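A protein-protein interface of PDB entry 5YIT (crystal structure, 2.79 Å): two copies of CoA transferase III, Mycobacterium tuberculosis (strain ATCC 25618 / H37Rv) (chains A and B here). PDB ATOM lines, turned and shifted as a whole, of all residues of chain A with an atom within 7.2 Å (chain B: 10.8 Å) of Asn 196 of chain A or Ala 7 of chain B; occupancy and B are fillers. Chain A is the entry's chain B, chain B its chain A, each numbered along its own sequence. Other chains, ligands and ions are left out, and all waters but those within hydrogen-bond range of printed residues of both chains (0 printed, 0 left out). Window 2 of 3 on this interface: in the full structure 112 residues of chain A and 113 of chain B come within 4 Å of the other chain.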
ATOM      1  N   LEU A 190       8.301 -21.205 -19.865  1.00  0.00           N
ATOM      2  CA  LEU A 190       9.702 -21.547 -20.049  1.00  0.00           C
ATOM      3  C   LEU A 190      10.592 -20.809 -19.058  1.00  0.00           C
ATOM      4  O   LEU A 190      11.506 -21.402 -18.475  1.00  0.00           O
ATOM      5  CB  LEU A 190      10.145 -21.280 -21.489  1.00  0.00           C
ATOM      6  CG  LEU A 190       9.758 -22.304 -22.566  1.00  0.00           C
ATOM      7  CD1 LEU A 190      10.187 -21.815 -23.935  1.00  0.00           C
ATOM      8  CD2 LEU A 190      10.320 -23.694 -22.310  1.00  0.00           C
ATOM      9  N   LEU A 191      10.300 -19.532 -18.842  1.00  0.00           N
ATOM     10  CA  LEU A 191      11.009 -18.747 -17.816  1.00  0.00           C
ATOM     11  C   LEU A 191      10.745 -19.287 -16.424  1.00  0.00           C
ATOM     12  O   LEU A 191      11.635 -19.352 -15.595  1.00  0.00           O
ATOM     13  CB  LEU A 191      10.608 -17.267 -17.856  1.00  0.00           C
ATOM     14  CG  LEU A 191      11.657 -16.371 -18.491  1.00  0.00           C
ATOM     15  CD1 LEU A 191      11.136 -14.944 -18.578  1.00  0.00           C
ATOM     16  CD2 LEU A 191      12.967 -16.480 -17.728  1.00  0.00           C
ATOM     17  N   HIS A 192       9.504 -19.700 -16.199  1.00  0.00           N
ATOM     18  CA  HIS A 192       9.076 -20.259 -14.933  1.00  0.00           C
ATOM     19  C   HIS A 192       9.851 -21.519 -14.631  1.00  0.00           C
ATOM     20  O   HIS A 192      10.303 -21.708 -13.519  1.00  0.00           O
ATOM     21  CB  HIS A 192       7.575 -20.597 -14.989  1.00  0.00           C
ATOM     22  CG  HIS A 192       6.943 -20.816 -13.645  1.00  0.00           C
ATOM     23  ND1 HIS A 192       7.419 -20.218 -12.501  1.00  0.00           N
ATOM     24  CD2 HIS A 192       5.840 -21.512 -13.276  1.00  0.00           C
ATOM     25  CE1 HIS A 192       6.654 -20.554 -11.482  1.00  0.00           C
ATOM     26  NE2 HIS A 192       5.687 -21.335 -11.926  1.00  0.00           N
ATOM     27  N   ARG A 193      10.019 -22.381 -15.631  1.00  0.00           N
ATOM     28  CA  ARG A 193      10.765 -23.618 -15.461  1.00  0.00           C
ATOM     29  C   ARG A 193      12.246 -23.348 -15.300  1.00  0.00           C
ATOM     30  O   ARG A 193      12.922 -24.044 -14.563  1.00  0.00           O
ATOM     31  CB  ARG A 193      10.522 -24.542 -16.635  1.00  0.00           C
ATOM     32  CG  ARG A 193      10.950 -25.982 -16.424  1.00  0.00           C
ATOM     33  CD  ARG A 193      11.049 -26.714 -17.755  1.00  0.00           C
ATOM     34  NE  ARG A 193      12.036 -26.087 -18.628  1.00  0.00           N
ATOM     35  CZ  ARG A 193      12.398 -26.551 -19.820  1.00  0.00           C
ATOM     36  NH1 ARG A 193      11.858 -27.662 -20.317  1.00  0.00           N
ATOM     37  NH2 ARG A 193      13.304 -25.879 -20.514  1.00  0.00           N
ATOM     38  N   GLU A 194      12.744 -22.310 -15.961  1.00  0.00           N
ATOM     39  CA  GLU A 194      14.157 -21.939 -15.859  1.00  0.00           C
ATOM     40  C   GLU A 194      14.518 -21.368 -14.493  1.00  0.00           C
ATOM     41  O   GLU A 194      15.565 -21.685 -13.973  1.00  0.00           O
ATOM     42  CB  GLU A 194      14.546 -20.946 -16.948  1.00  0.00           C
ATOM     43  CG  GLU A 194      14.716 -21.564 -18.327  1.00  0.00           C
ATOM     44  CD  GLU A 194      15.842 -22.580 -18.401  1.00  0.00           C
ATOM     45  OE1 GLU A 194      16.882 -22.354 -17.754  1.00  0.00           O
ATOM     46  OE2 GLU A 194      15.684 -23.599 -19.115  1.00  0.00           O
ATOM     47  N   ARG A 195      13.654 -20.546 -13.902  1.00  0.00           N
ATOM     48  CA  ARG A 195      14.003 -19.837 -12.669  1.00  0.00           C
ATOM     49  C   ARG A 195      13.351 -20.412 -11.434  1.00  0.00           C
ATOM     50  O   ARG A 195      13.737 -20.072 -10.333  1.00  0.00           O
ATOM     51  CB  ARG A 195      13.673 -18.340 -12.779  1.00  0.00           C
ATOM     52  CG  ARG A 195      14.455 -17.630 -13.854  1.00  0.00           C
ATOM     53  CD  ARG A 195      13.980 -16.206 -13.983  1.00  0.00           C
ATOM     54  NE  ARG A 195      14.564 -15.320 -12.986  1.00  0.00           N
ATOM     55  CZ  ARG A 195      13.882 -14.712 -12.016  1.00  0.00           C
ATOM     56  NH1 ARG A 195      12.552 -14.885 -11.876  1.00  0.00           N
ATOM     57  NH2 ARG A 195      14.542 -13.908 -11.184  1.00  0.00           N
ATOM     58  N   ASN A 196      12.353 -21.255 -11.611  1.00  0.00           N
ATOM     59  CA  ASN A 196      11.673 -21.858 -10.471  1.00  0.00           C
ATOM     60  C   ASN A 196      11.571 -23.369 -10.576  1.00  0.00           C
ATOM     61  O   ASN A 196      11.019 -24.019  -9.694  1.00  0.00           O
ATOM     62  CB  ASN A 196      10.286 -21.234 -10.251  1.00  0.00           C
ATOM     63  CG  ASN A 196      10.354 -19.733 -10.032  1.00  0.00           C
ATOM     64  OD1 ASN A 196      11.165 -19.247  -9.237  1.00  0.00           O
ATOM     65  ND2 ASN A 196       9.528 -18.983 -10.759  1.00  0.00           N
ATOM     66  N   GLY A 197      12.105 -23.926 -11.658  1.00  0.00           N
ATOM     67  CA  GLY A 197      12.058 -25.358 -11.886  1.00  0.00           C
ATOM     68  C   GLY A 197      10.647 -25.896 -11.865  1.00  0.00           C
ATOM     69  O   GLY A 197      10.410 -26.947 -11.270  1.00  0.00           O
ATOM     70  N   VAL A 198       9.703 -25.183 -12.492  1.00  0.00           N
ATOM     71  CA  VAL A 198       8.324 -25.698 -12.573  1.00  0.00           C
ATOM     72  C   VAL A 198       7.886 -25.929 -13.992  1.00  0.00           C
ATOM     73  O   VAL A 198       7.994 -25.073 -14.827  1.00  0.00           O
ATOM     74  CB  VAL A 198       7.299 -24.788 -11.909  1.00  0.00           C
ATOM     75  CG1 VAL A 198       6.044 -25.580 -11.580  1.00  0.00           C
ATOM     76  CG2 VAL A 198       7.884 -24.158 -10.658  1.00  0.00           C
ATOM     77  N   ALA A 199       7.375 -27.110 -14.256  1.00  0.00           N
ATOM     78  CA  ALA A 199       6.930 -27.402 -15.581  1.00  0.00           C
ATOM     79  C   ALA A 199       5.467 -27.184 -15.516  1.00  0.00           C
ATOM     80  O   ALA A 199       4.754 -28.073 -15.107  1.00  0.00           O
ATOM     81  CB  ALA A 199       7.224 -28.841 -15.943  1.00  0.00           C
ATOM     82  N   ASP A 200       5.017 -26.008 -15.926  1.00  0.00           N
ATOM     83  CA  ASP A 200       3.619 -25.667 -15.798  1.00  0.00           C
ATOM     84  C   ASP A 200       2.681 -26.228 -16.863  1.00  0.00           C
ATOM     85  O   ASP A 200       3.128 -26.710 -17.911  1.00  0.00           O
ATOM     86  CB  ASP A 200       3.465 -24.170 -15.702  1.00  0.00           C
ATOM     87  CG  ASP A 200       2.464 -23.781 -14.653  1.00  0.00           C
ATOM     88  OD1 ASP A 200       1.512 -24.565 -14.429  1.00  0.00           O
ATOM     89  OD2 ASP A 200       2.635 -22.698 -14.048  1.00  0.00           O
ATOM     90  N   ASN B   5       0.740 -18.714  -1.726  1.00  0.00           N
ATOM     91  CA  ASN B   5       1.905 -17.890  -2.026  1.00  0.00           C
ATOM     92  C   ASN B   5       3.016 -18.716  -2.664  1.00  0.00           C
ATOM     93  O   ASN B   5       3.999 -19.062  -2.009  1.00  0.00           O
ATOM     94  CB  ASN B   5       2.407 -17.204  -0.765  1.00  0.00           C
ATOM     95  N   PRO B   6       2.853 -19.028  -3.945  1.00  0.00           N
ATOM     96  CA  PRO B   6       3.847 -19.819  -4.678  1.00  0.00           C
ATOM     97  C   PRO B   6       4.710 -18.946  -5.583  1.00  0.00           C
ATOM     98  O   PRO B   6       4.355 -17.800  -5.856  1.00  0.00           O
ATOM     99  CB  PRO B   6       2.987 -20.761  -5.523  1.00  0.00           C
ATOM    100  CG  PRO B   6       1.715 -20.010  -5.731  1.00  0.00           C
ATOM    101  CD  PRO B   6       1.490 -19.226  -4.468  1.00  0.00           C
ATOM    102  N   ALA B   7       5.834 -19.490  -6.040  1.00  0.00           N
ATOM    103  CA  ALA B   7       6.740 -18.757  -6.911  1.00  0.00           C
ATOM    104  C   ALA B   7       6.108 -18.525  -8.262  1.00  0.00           C
ATOM    105  O   ALA B   7       5.457 -19.408  -8.794  1.00  0.00           O
ATOM    106  CB  ALA B   7       8.059 -19.457  -7.060  1.00  0.00           C
ATOM    107  N   LYS B   8       6.265 -17.303  -8.763  1.00  0.00           N
ATOM    108  CA  LYS B   8       5.781 -16.895 -10.077  1.00  0.00           C
ATOM    109  C   LYS B   8       6.979 -16.670 -10.999  1.00  0.00           C
ATOM    110  O   LYS B   8       8.090 -16.394 -10.521  1.00  0.00           O
ATOM    111  CB  LYS B   8       4.972 -15.608  -9.991  1.00  0.00           C
ATOM    112  CG  LYS B   8       3.592 -15.799  -9.456  1.00  0.00           C
ATOM    113  CD  LYS B   8       2.866 -14.468  -9.483  1.00  0.00           C
ATOM    114  CE  LYS B   8       1.411 -14.621  -9.055  1.00  0.00           C
ATOM    115  NZ  LYS B   8       0.706 -13.310  -9.134  1.00  0.00           N
ATOM    116  N   PRO B   9       6.761 -16.785 -12.331  1.00  0.00           N
ATOM    117  CA  PRO B   9       7.854 -16.786 -13.291  1.00  0.00           C
ATOM    118  C   PRO B   9       8.734 -15.542 -13.219  1.00  0.00           C
ATOM    119  O   PRO B   9       9.960 -15.634 -13.380  1.00  0.00           O
ATOM    120  CB  PRO B   9       7.129 -16.845 -14.620  1.00  0.00           C
ATOM    121  CG  PRO B   9       5.844 -17.515 -14.316  1.00  0.00           C
ATOM    122  CD  PRO B   9       5.464 -16.990 -12.993  1.00  0.00           C
ATOM    123  N   LEU B  10       8.125 -14.395 -12.968  1.00  0.00           N
ATOM    124  CA  LEU B  10       8.874 -13.141 -13.003  1.00  0.00           C
ATOM    125  C   LEU B  10       9.211 -12.600 -11.628  1.00  0.00           C
ATOM    126  O   LEU B  10       9.470 -11.420 -11.494  1.00  0.00           O
ATOM    127  CB  LEU B  10       8.133 -12.091 -13.849  1.00  0.00           C
ATOM    128  CG  LEU B  10       7.783 -12.496 -15.273  1.00  0.00           C
ATOM    129  CD1 LEU B  10       7.189 -11.292 -15.986  1.00  0.00           C
ATOM    130  CD2 LEU B  10       9.003 -13.044 -16.010  1.00  0.00           C
ATOM    131  N   ASP B  11       9.194 -13.459 -10.611  1.00  0.00           N
ATOM    132  CA  ASP B  11       9.546 -13.046  -9.250  1.00  0.00           C
ATOM    133  C   ASP B  11      10.985 -12.572  -9.190  1.00  0.00           C
ATOM    134  O   ASP B  11      11.888 -13.232  -9.707  1.00  0.00           O
ATOM    135  CB  ASP B  11       9.328 -14.183  -8.255  1.00  0.00           C
ATOM    136  CG  ASP B  11       7.915 -14.198  -7.673  1.00  0.00           C
ATOM    137  OD1 ASP B  11       7.176 -13.188  -7.791  1.00  0.00           O
ATOM    138  OD2 ASP B  11       7.539 -15.235  -7.084  1.00  0.00           O
ATOM    139  N   GLY B  12      11.190 -11.401  -8.604  1.00  0.00           N
ATOM    140  CA  GLY B  12      12.522 -10.818  -8.513  1.00  0.00           C
ATOM    141  C   GLY B  12      12.963 -10.059  -9.748  1.00  0.00           C
ATOM    142  O   GLY B  12      14.142  -9.740  -9.900  1.00  0.00           O
ATOM    143  N   PHE B  13      12.017  -9.763 -10.634  1.00  0.00           N
ATOM    144  CA  PHE B  13      12.276  -8.917 -11.786  1.00  0.00           C
ATOM    145  C   PHE B  13      11.685  -7.519 -11.574  1.00  0.00           C
ATOM    146  O   PHE B  13      10.636  -7.371 -10.944  1.00  0.00           O
ATOM    147  CB  PHE B  13      11.722  -9.542 -13.062  1.00  0.00           C
ATOM    148  CG  PHE B  13      12.541 -10.683 -13.617  1.00  0.00           C
ATOM    149  CD1 PHE B  13      13.934 -10.640 -13.652  1.00  0.00           C
ATOM    150  CD2 PHE B  13      11.900 -11.781 -14.185  1.00  0.00           C
ATOM    151  CE1 PHE B  13      14.672 -11.682 -14.196  1.00  0.00           C
ATOM    152  CE2 PHE B  13      12.629 -12.815 -14.757  1.00  0.00           C
ATOM    153  CZ  PHE B  13      14.021 -12.767 -14.767  1.00  0.00           C
ATOM    154  N   VAL B  32       2.994  -7.831 -14.393  1.00  0.00           N
ATOM    155  CA  VAL B  32       2.565  -7.847 -12.994  1.00  0.00           C
ATOM    156  C   VAL B  32       1.902  -9.154 -12.599  1.00  0.00           C
ATOM    157  O   VAL B  32       2.221  -9.719 -11.556  1.00  0.00           O
ATOM    158  CB  VAL B  32       1.641  -6.671 -12.682  1.00  0.00           C
ATOM    159  CG1 VAL B  32       0.847  -6.929 -11.416  1.00  0.00           C
ATOM    160  CG2 VAL B  32       2.448  -5.396 -12.505  1.00  0.00           C
ATOM    161  N   ASP B  33       1.003  -9.630 -13.455  1.00  0.00           N
ATOM    162  CA  ASP B  33       0.305 -10.885 -13.238  1.00  0.00           C
ATOM    163  C   ASP B  33       1.284 -12.065 -13.176  1.00  0.00           C
ATOM    164  O   ASP B  33       1.024 -13.078 -12.515  1.00  0.00           O
ATOM    165  CB  ASP B  33      -0.737 -11.121 -14.335  1.00  0.00           C
ATOM    166  CG  ASP B  33      -1.925 -10.213 -14.200  1.00  0.00           C
ATOM    167  OD1 ASP B  33      -1.753  -9.068 -13.755  1.00  0.00           O
ATOM    168  OD2 ASP B  33      -3.049 -10.635 -14.506  1.00  0.00           O
ATOM    169  N   LEU B  34       2.404 -11.926 -13.871  1.00  0.00           N
ATOM    170  CA  LEU B  34       3.410 -12.977 -13.904  1.00  0.00           C
ATOM    171  C   LEU B  34       4.437 -12.815 -12.784  1.00  0.00           C
ATOM    172  O   LEU B  34       5.409 -13.584 -12.719  1.00  0.00           O
ATOM    173  CB  LEU B  34       4.089 -13.048 -15.285  1.00  0.00           C
ATOM    174  CG  LEU B  34       3.125 -13.471 -16.392  1.00  0.00           C
ATOM    175  CD1 LEU B  34       3.869 -13.413 -17.696  1.00  0.00           C
ATOM    176  CD2 LEU B  34       2.456 -14.829 -16.139  1.00  0.00           C
ATOM    177  N   GLY B  35       4.214 -11.821 -11.917  1.00  0.00           N
ATOM    178  CA  GLY B  35       4.965 -11.676 -10.686  1.00  0.00           C
ATOM    179  C   GLY B  35       6.109 -10.677 -10.696  1.00  0.00           C
ATOM    180  O   GLY B  35       6.821 -10.517  -9.692  1.00  0.00           O
ATOM    181  N   ALA B  36       6.288  -9.981 -11.811  1.00  0.00           N
ATOM    182  CA  ALA B  36       7.305  -8.937 -11.883  1.00  0.00           C
ATOM    183  C   ALA B  36       6.885  -7.721 -11.065  1.00  0.00           C
ATOM    184  O   ALA B  36       5.694  -7.483 -10.861  1.00  0.00           O
ATOM    185  CB  ALA B  36       7.542  -8.529 -13.313  1.00  0.00           C
ATOM    186  N   LEU B 191      14.173 -14.337 -21.516  1.00  0.00           N
ATOM    187  CA  LEU B 191      14.629 -15.676 -21.748  1.00  0.00           C
ATOM    188  C   LEU B 191      15.943 -15.611 -22.498  1.00  0.00           C
ATOM    189  O   LEU B 191      16.839 -16.386 -22.248  1.00  0.00           O
ATOM    190  CB  LEU B 191      13.582 -16.385 -22.570  1.00  0.00           C
ATOM    191  CG  LEU B 191      13.447 -17.870 -22.358  1.00  0.00           C
ATOM    192  CD1 LEU B 191      13.880 -18.235 -20.949  1.00  0.00           C
ATOM    193  CD2 LEU B 191      11.990 -18.214 -22.597  1.00  0.00           C
ATOM    194  N   GLU B 194      18.564 -14.750 -20.114  1.00  0.00           N
ATOM    195  CA  GLU B 194      18.767 -15.880 -19.206  1.00  0.00           C
ATOM    196  C   GLU B 194      19.630 -16.983 -19.798  1.00  0.00           C
ATOM    197  O   GLU B 194      20.511 -17.508 -19.124  1.00  0.00           O
ATOM    198  CB  GLU B 194      17.437 -16.458 -18.747  1.00  0.00           C
ATOM    199  CG  GLU B 194      17.498 -17.028 -17.332  1.00  0.00           C
ATOM    200  CD  GLU B 194      17.812 -15.972 -16.273  1.00  0.00           C
ATOM    201  OE1 GLU B 194      17.320 -14.809 -16.361  1.00  0.00           O
ATOM    202  OE2 GLU B 194      18.558 -16.320 -15.339  1.00  0.00           O
ATOM    203  N   TYR B 369      -2.377 -20.385 -15.850  1.00  0.00           N
ATOM    204  CA  TYR B 369      -1.358 -21.335 -15.448  1.00  0.00           C
ATOM    205  C   TYR B 369      -1.844 -22.196 -14.309  1.00  0.00           C
ATOM    206  O   TYR B 369      -2.795 -21.842 -13.594  1.00  0.00           O
ATOM    207  CB  TYR B 369      -0.099 -20.587 -15.072  1.00  0.00           C
ATOM    208  CG  TYR B 369       0.341 -19.617 -16.137  1.00  0.00           C
ATOM    209  CD1 TYR B 369      -0.331 -18.401 -16.330  1.00  0.00           C
ATOM    210  CD2 TYR B 369       1.415 -19.912 -16.962  1.00  0.00           C
ATOM    211  CE1 TYR B 369       0.036 -17.532 -17.316  1.00  0.00           C
ATOM    212  CE2 TYR B 369       1.818 -19.017 -17.930  1.00  0.00           C
ATOM    213  CZ  TYR B 369       1.117 -17.840 -18.096  1.00  0.00           C
ATOM    214  OH  TYR B 369       1.500 -16.950 -19.057  1.00  0.00           O
ATOM    215  N   ALA B 370      -1.205 -23.348 -14.139  1.00  0.00           N
ATOM    216  CA  ALA B 370      -1.605 -24.283 -13.092  1.00  0.00           C
ATOM    217  C   ALA B 370      -0.847 -24.036 -11.795  1.00  0.00           C
ATOM    218  O   ALA B 370      -1.444 -24.075 -10.735  1.00  0.00           O
ATOM    219  CB  ALA B 370      -1.419 -25.722 -13.558  1.00  0.00           C
ATOM    220  N   SER B 371       0.454 -23.782 -11.889  1.00  0.00           N
ATOM    221  CA  SER B 371       1.286 -23.703 -10.715  1.00  0.00           C
ATOM    222  C   SER B 371       0.932 -22.502  -9.888  1.00  0.00           C
ATOM    223  O   SER B 371       1.115 -22.520  -8.677  1.00  0.00           O
ATOM    224  CB  SER B 371       2.772 -23.701 -11.081  1.00  0.00           C
ATOM    225  OG  SER B 371       3.260 -22.398 -11.330  1.00  0.00           O
ATOM    226  N   PHE B 372       0.437 -21.451 -10.537  1.00  0.00           N
ATOM    227  CA  PHE B 372       0.018 -20.242  -9.841  1.00  0.00           C
ATOM    228  C   PHE B 372      -1.168 -19.582 -10.510  1.00  0.00           C
ATOM    229  O   PHE B 372      -1.543 -19.962 -11.599  1.00  0.00           O
ATOM    230  CB  PHE B 372       1.169 -19.274  -9.802  1.00  0.00           C
ATOM    231  CG  PHE B 372       1.502 -18.706 -11.123  1.00  0.00           C
ATOM    232  CD1 PHE B 372       2.306 -19.421 -12.016  1.00  0.00           C
ATOM    233  CD2 PHE B 372       1.037 -17.439 -11.476  1.00  0.00           C
ATOM    234  CE1 PHE B 372       2.639 -18.881 -13.239  1.00  0.00           C
ATOM    235  CE2 PHE B 372       1.367 -16.897 -12.700  1.00  0.00           C
ATOM    236  CZ  PHE B 372       2.166 -17.607 -13.582  1.00  0.00           C
ATOM    237  N   ARG B 373      -1.757 -18.586  -9.865  1.00  0.00           N
ATOM    238  CA  ARG B 373      -2.857 -17.841 -10.479  1.00  0.00           C
ATOM    239  C   ARG B 373      -2.331 -16.496 -10.971  1.00  0.00           C
ATOM    240  O   ARG B 373      -1.839 -15.708 -10.168  1.00  0.00           O
ATOM    241  CB  ARG B 373      -4.019 -17.666  -9.506  1.00  0.00           C
ATOM    242  N   ALA B 374      -2.409 -16.249 -12.282  1.00  0.00           N
ATOM    243  CA  ALA B 374      -1.853 -15.000 -12.843  1.00  0.00           C
ATOM    244  C   ALA B 374      -2.833 -13.859 -12.728  1.00  0.00           C
ATOM    245  O   ALA B 374      -3.340 -13.349 -13.731  1.00  0.00           O
ATOM    246  CB  ALA B 374      -1.434 -15.172 -14.278  1.00  0.00           C
ATOM    247  N   VAL B 375      -3.106 -13.485 -11.485  1.00  0.00           N
ATOM    248  CA  VAL B 375      -4.057 -12.431 -11.145  1.00  0.00           C
ATOM    249  C   VAL B 375      -3.501 -11.726  -9.936  1.00  0.00           C
ATOM    250  O   VAL B 375      -2.850 -12.355  -9.104  1.00  0.00           O
ATOM    251  CB  VAL B 375      -5.470 -12.981 -10.799  1.00  0.00           C
ATOM    252  CG1 VAL B 375      -5.898 -14.074 -11.769  1.00  0.00           C
ATOM    253  CG2 VAL B 375      -5.540 -13.515  -9.369  1.00  0.00           C
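The side-chain carboxylate (OD2) of Asp 11 of chain B lies within hydrogen-bond range of the backbone NH (N) of Lys 8 of chain B (3.0 Å).
NZ of Lys 8 of chain B sits at hydrogen-bond distance from O of Asp 33 of chain B, at 3.4 Å.
The backbone NH of Leu 10 of chain B lies within hydrogen-bond range of the backbone carbonyl oxygen of Leu 34 of chain B, at 2.8 Å.
ND1 of His 192 of chain A lies within hydrogen-bond range of ND2 of Asn 196 of chain A.
The backbone carbonyl oxygen (O) of His 192 of chain A is in hydrogen-bond range of the backbone NH (N) of Gly 197 of chain A (3.4 Å).
The backbone NH of Arg 193 of chain A sits close to the backbone carbonyl oxygen of Val 198 of chain A.
The side-chain amide nitrogen (ND2) of Asn 196 of chain A sits at hydrogen-bond distance from the backbone carbonyl oxygen (O) of Lys 8 of chain B, at 3.0 Å.
The guanidinium group (NH1) of Arg 195 of chain A is in hydrogen-bond range of the backbone carbonyl oxygen (O) of Pro 9 of chain B (3.1 Å).
NH1 of Arg 195 of chain A sits at hydrogen-bond distance from O of Asp 11 of chain B.
N of Ala 370 of chain B is in hydrogen-bond range of OD1 of Asp 200 of chain A (3.0 Å).
The side-chain hydroxyl of Ser 371 of chain B sits at hydrogen-bond distance from a ring nitrogen (NE2) of His 192 of chain A (2.7 Å).
The side-chain hydroxyl of Ser 371 of chain B lies within hydrogen-bond range of the side-chain carboxylate of Asp 200 of chain A (2.8 Å).
ND1 of His 192 of chain A lies close to N of Pro 9 of chain B, 3.5 Å away.
Leu 191 of chain B touches its own counterpart, Leu 191 of chain A.
Positions printed for both chains: 191 and 194.
Of the 19 pairs that touch across the chains among the printed residues, 1 has its exchanged pair printed and touching as well.
Leu 191 of chain B touches Leu 190 of chain A (CD2 to CB, 3.7 Å).
CD1 of Leu 191 of chain A touches CD2 of Leu 10 of chain B (3.8 Å).
Leu 191 of chain A touches Leu 191 of chain B (CD2 to CD1, 3.8 Å).
NE2 of His 192 of chain A touches CD1 of Phe 372 of chain B (3.9 Å).
Arg 195 of chain A touches Phe 13 of chain B.
Ala 7 of chain B touches Asn 196 of chain A (CB to CG, 3.8 Å).
CA of Pro 9 of chain B touches ND2 of Asn 196 of chain A (3.7 Å).
CB of Ser 371 of chain B touches CG1 of Val 198 of chain A, at 3.8 Å.
Tyr 369 of chain B touches Asp 200 of chain A.
CD1 of Phe 372 of chain B touches OD2 of Asp 200 of chain A, at 3.9 Å.
His 192 of chain A touches just these residues of chain B: Ala 7 (3.2 Å), Lys 8 (3.9 Å), Pro 9 (3.5 Å), Ser 371 (2.7 Å) and Phe 372 (3.9 Å).
Arg 195 of chain A touches three residues of chain B.
Of chain B, only Ser 371 comes within 4 Å of Val 198 of chain A.
Printed residues of chain A within 4 Å of Tyr 369 of chain B: Asp 200.
Of the printed residues of chain A, Phe 13 of chain B touches Arg 195 (3.2 Å).
Printed residues of chain A within 4 Å of Pro 9 of chain B: His 192, Arg 195 and Asn 196.
Printed residues of chain A within 4 Å of Lys 8 of chain B: His 192 (3.9 Å) and Asn 196 (3.0 Å).
Glu 194 of chain B touches none of the printed residues of chain A.
The nearest residue of chain B that does not touch Asn 196 of chain A is Leu 10 of chain B (5.3 Å).
The nearest residue of chain A that does not touch Ala 7 of chain B is Val 198 of chain A (5.7 Å).
Hydrophobic or aromatic side chains of chain B within 4 Å of the printed part of chain A: Ala 7, Pro 9, Leu 10, Phe 13, Leu 191, Tyr 369, Ala 370 and Phe 372.
Of the 11 printed residues of chain A, 7 touch a printed residue of chain B.
Hydrophobic or aromatic side chains of chain A within 4 Å of the printed part of chain B: Leu 190, Leu 191, His 192 and Val 198.
Among the printed residues, 19 pairs touch across the chains.
Among the printed residues, no Asp or Glu carboxylate lies within 4 Å of a Lys or Arg side-chain nitrogen of the other chain.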
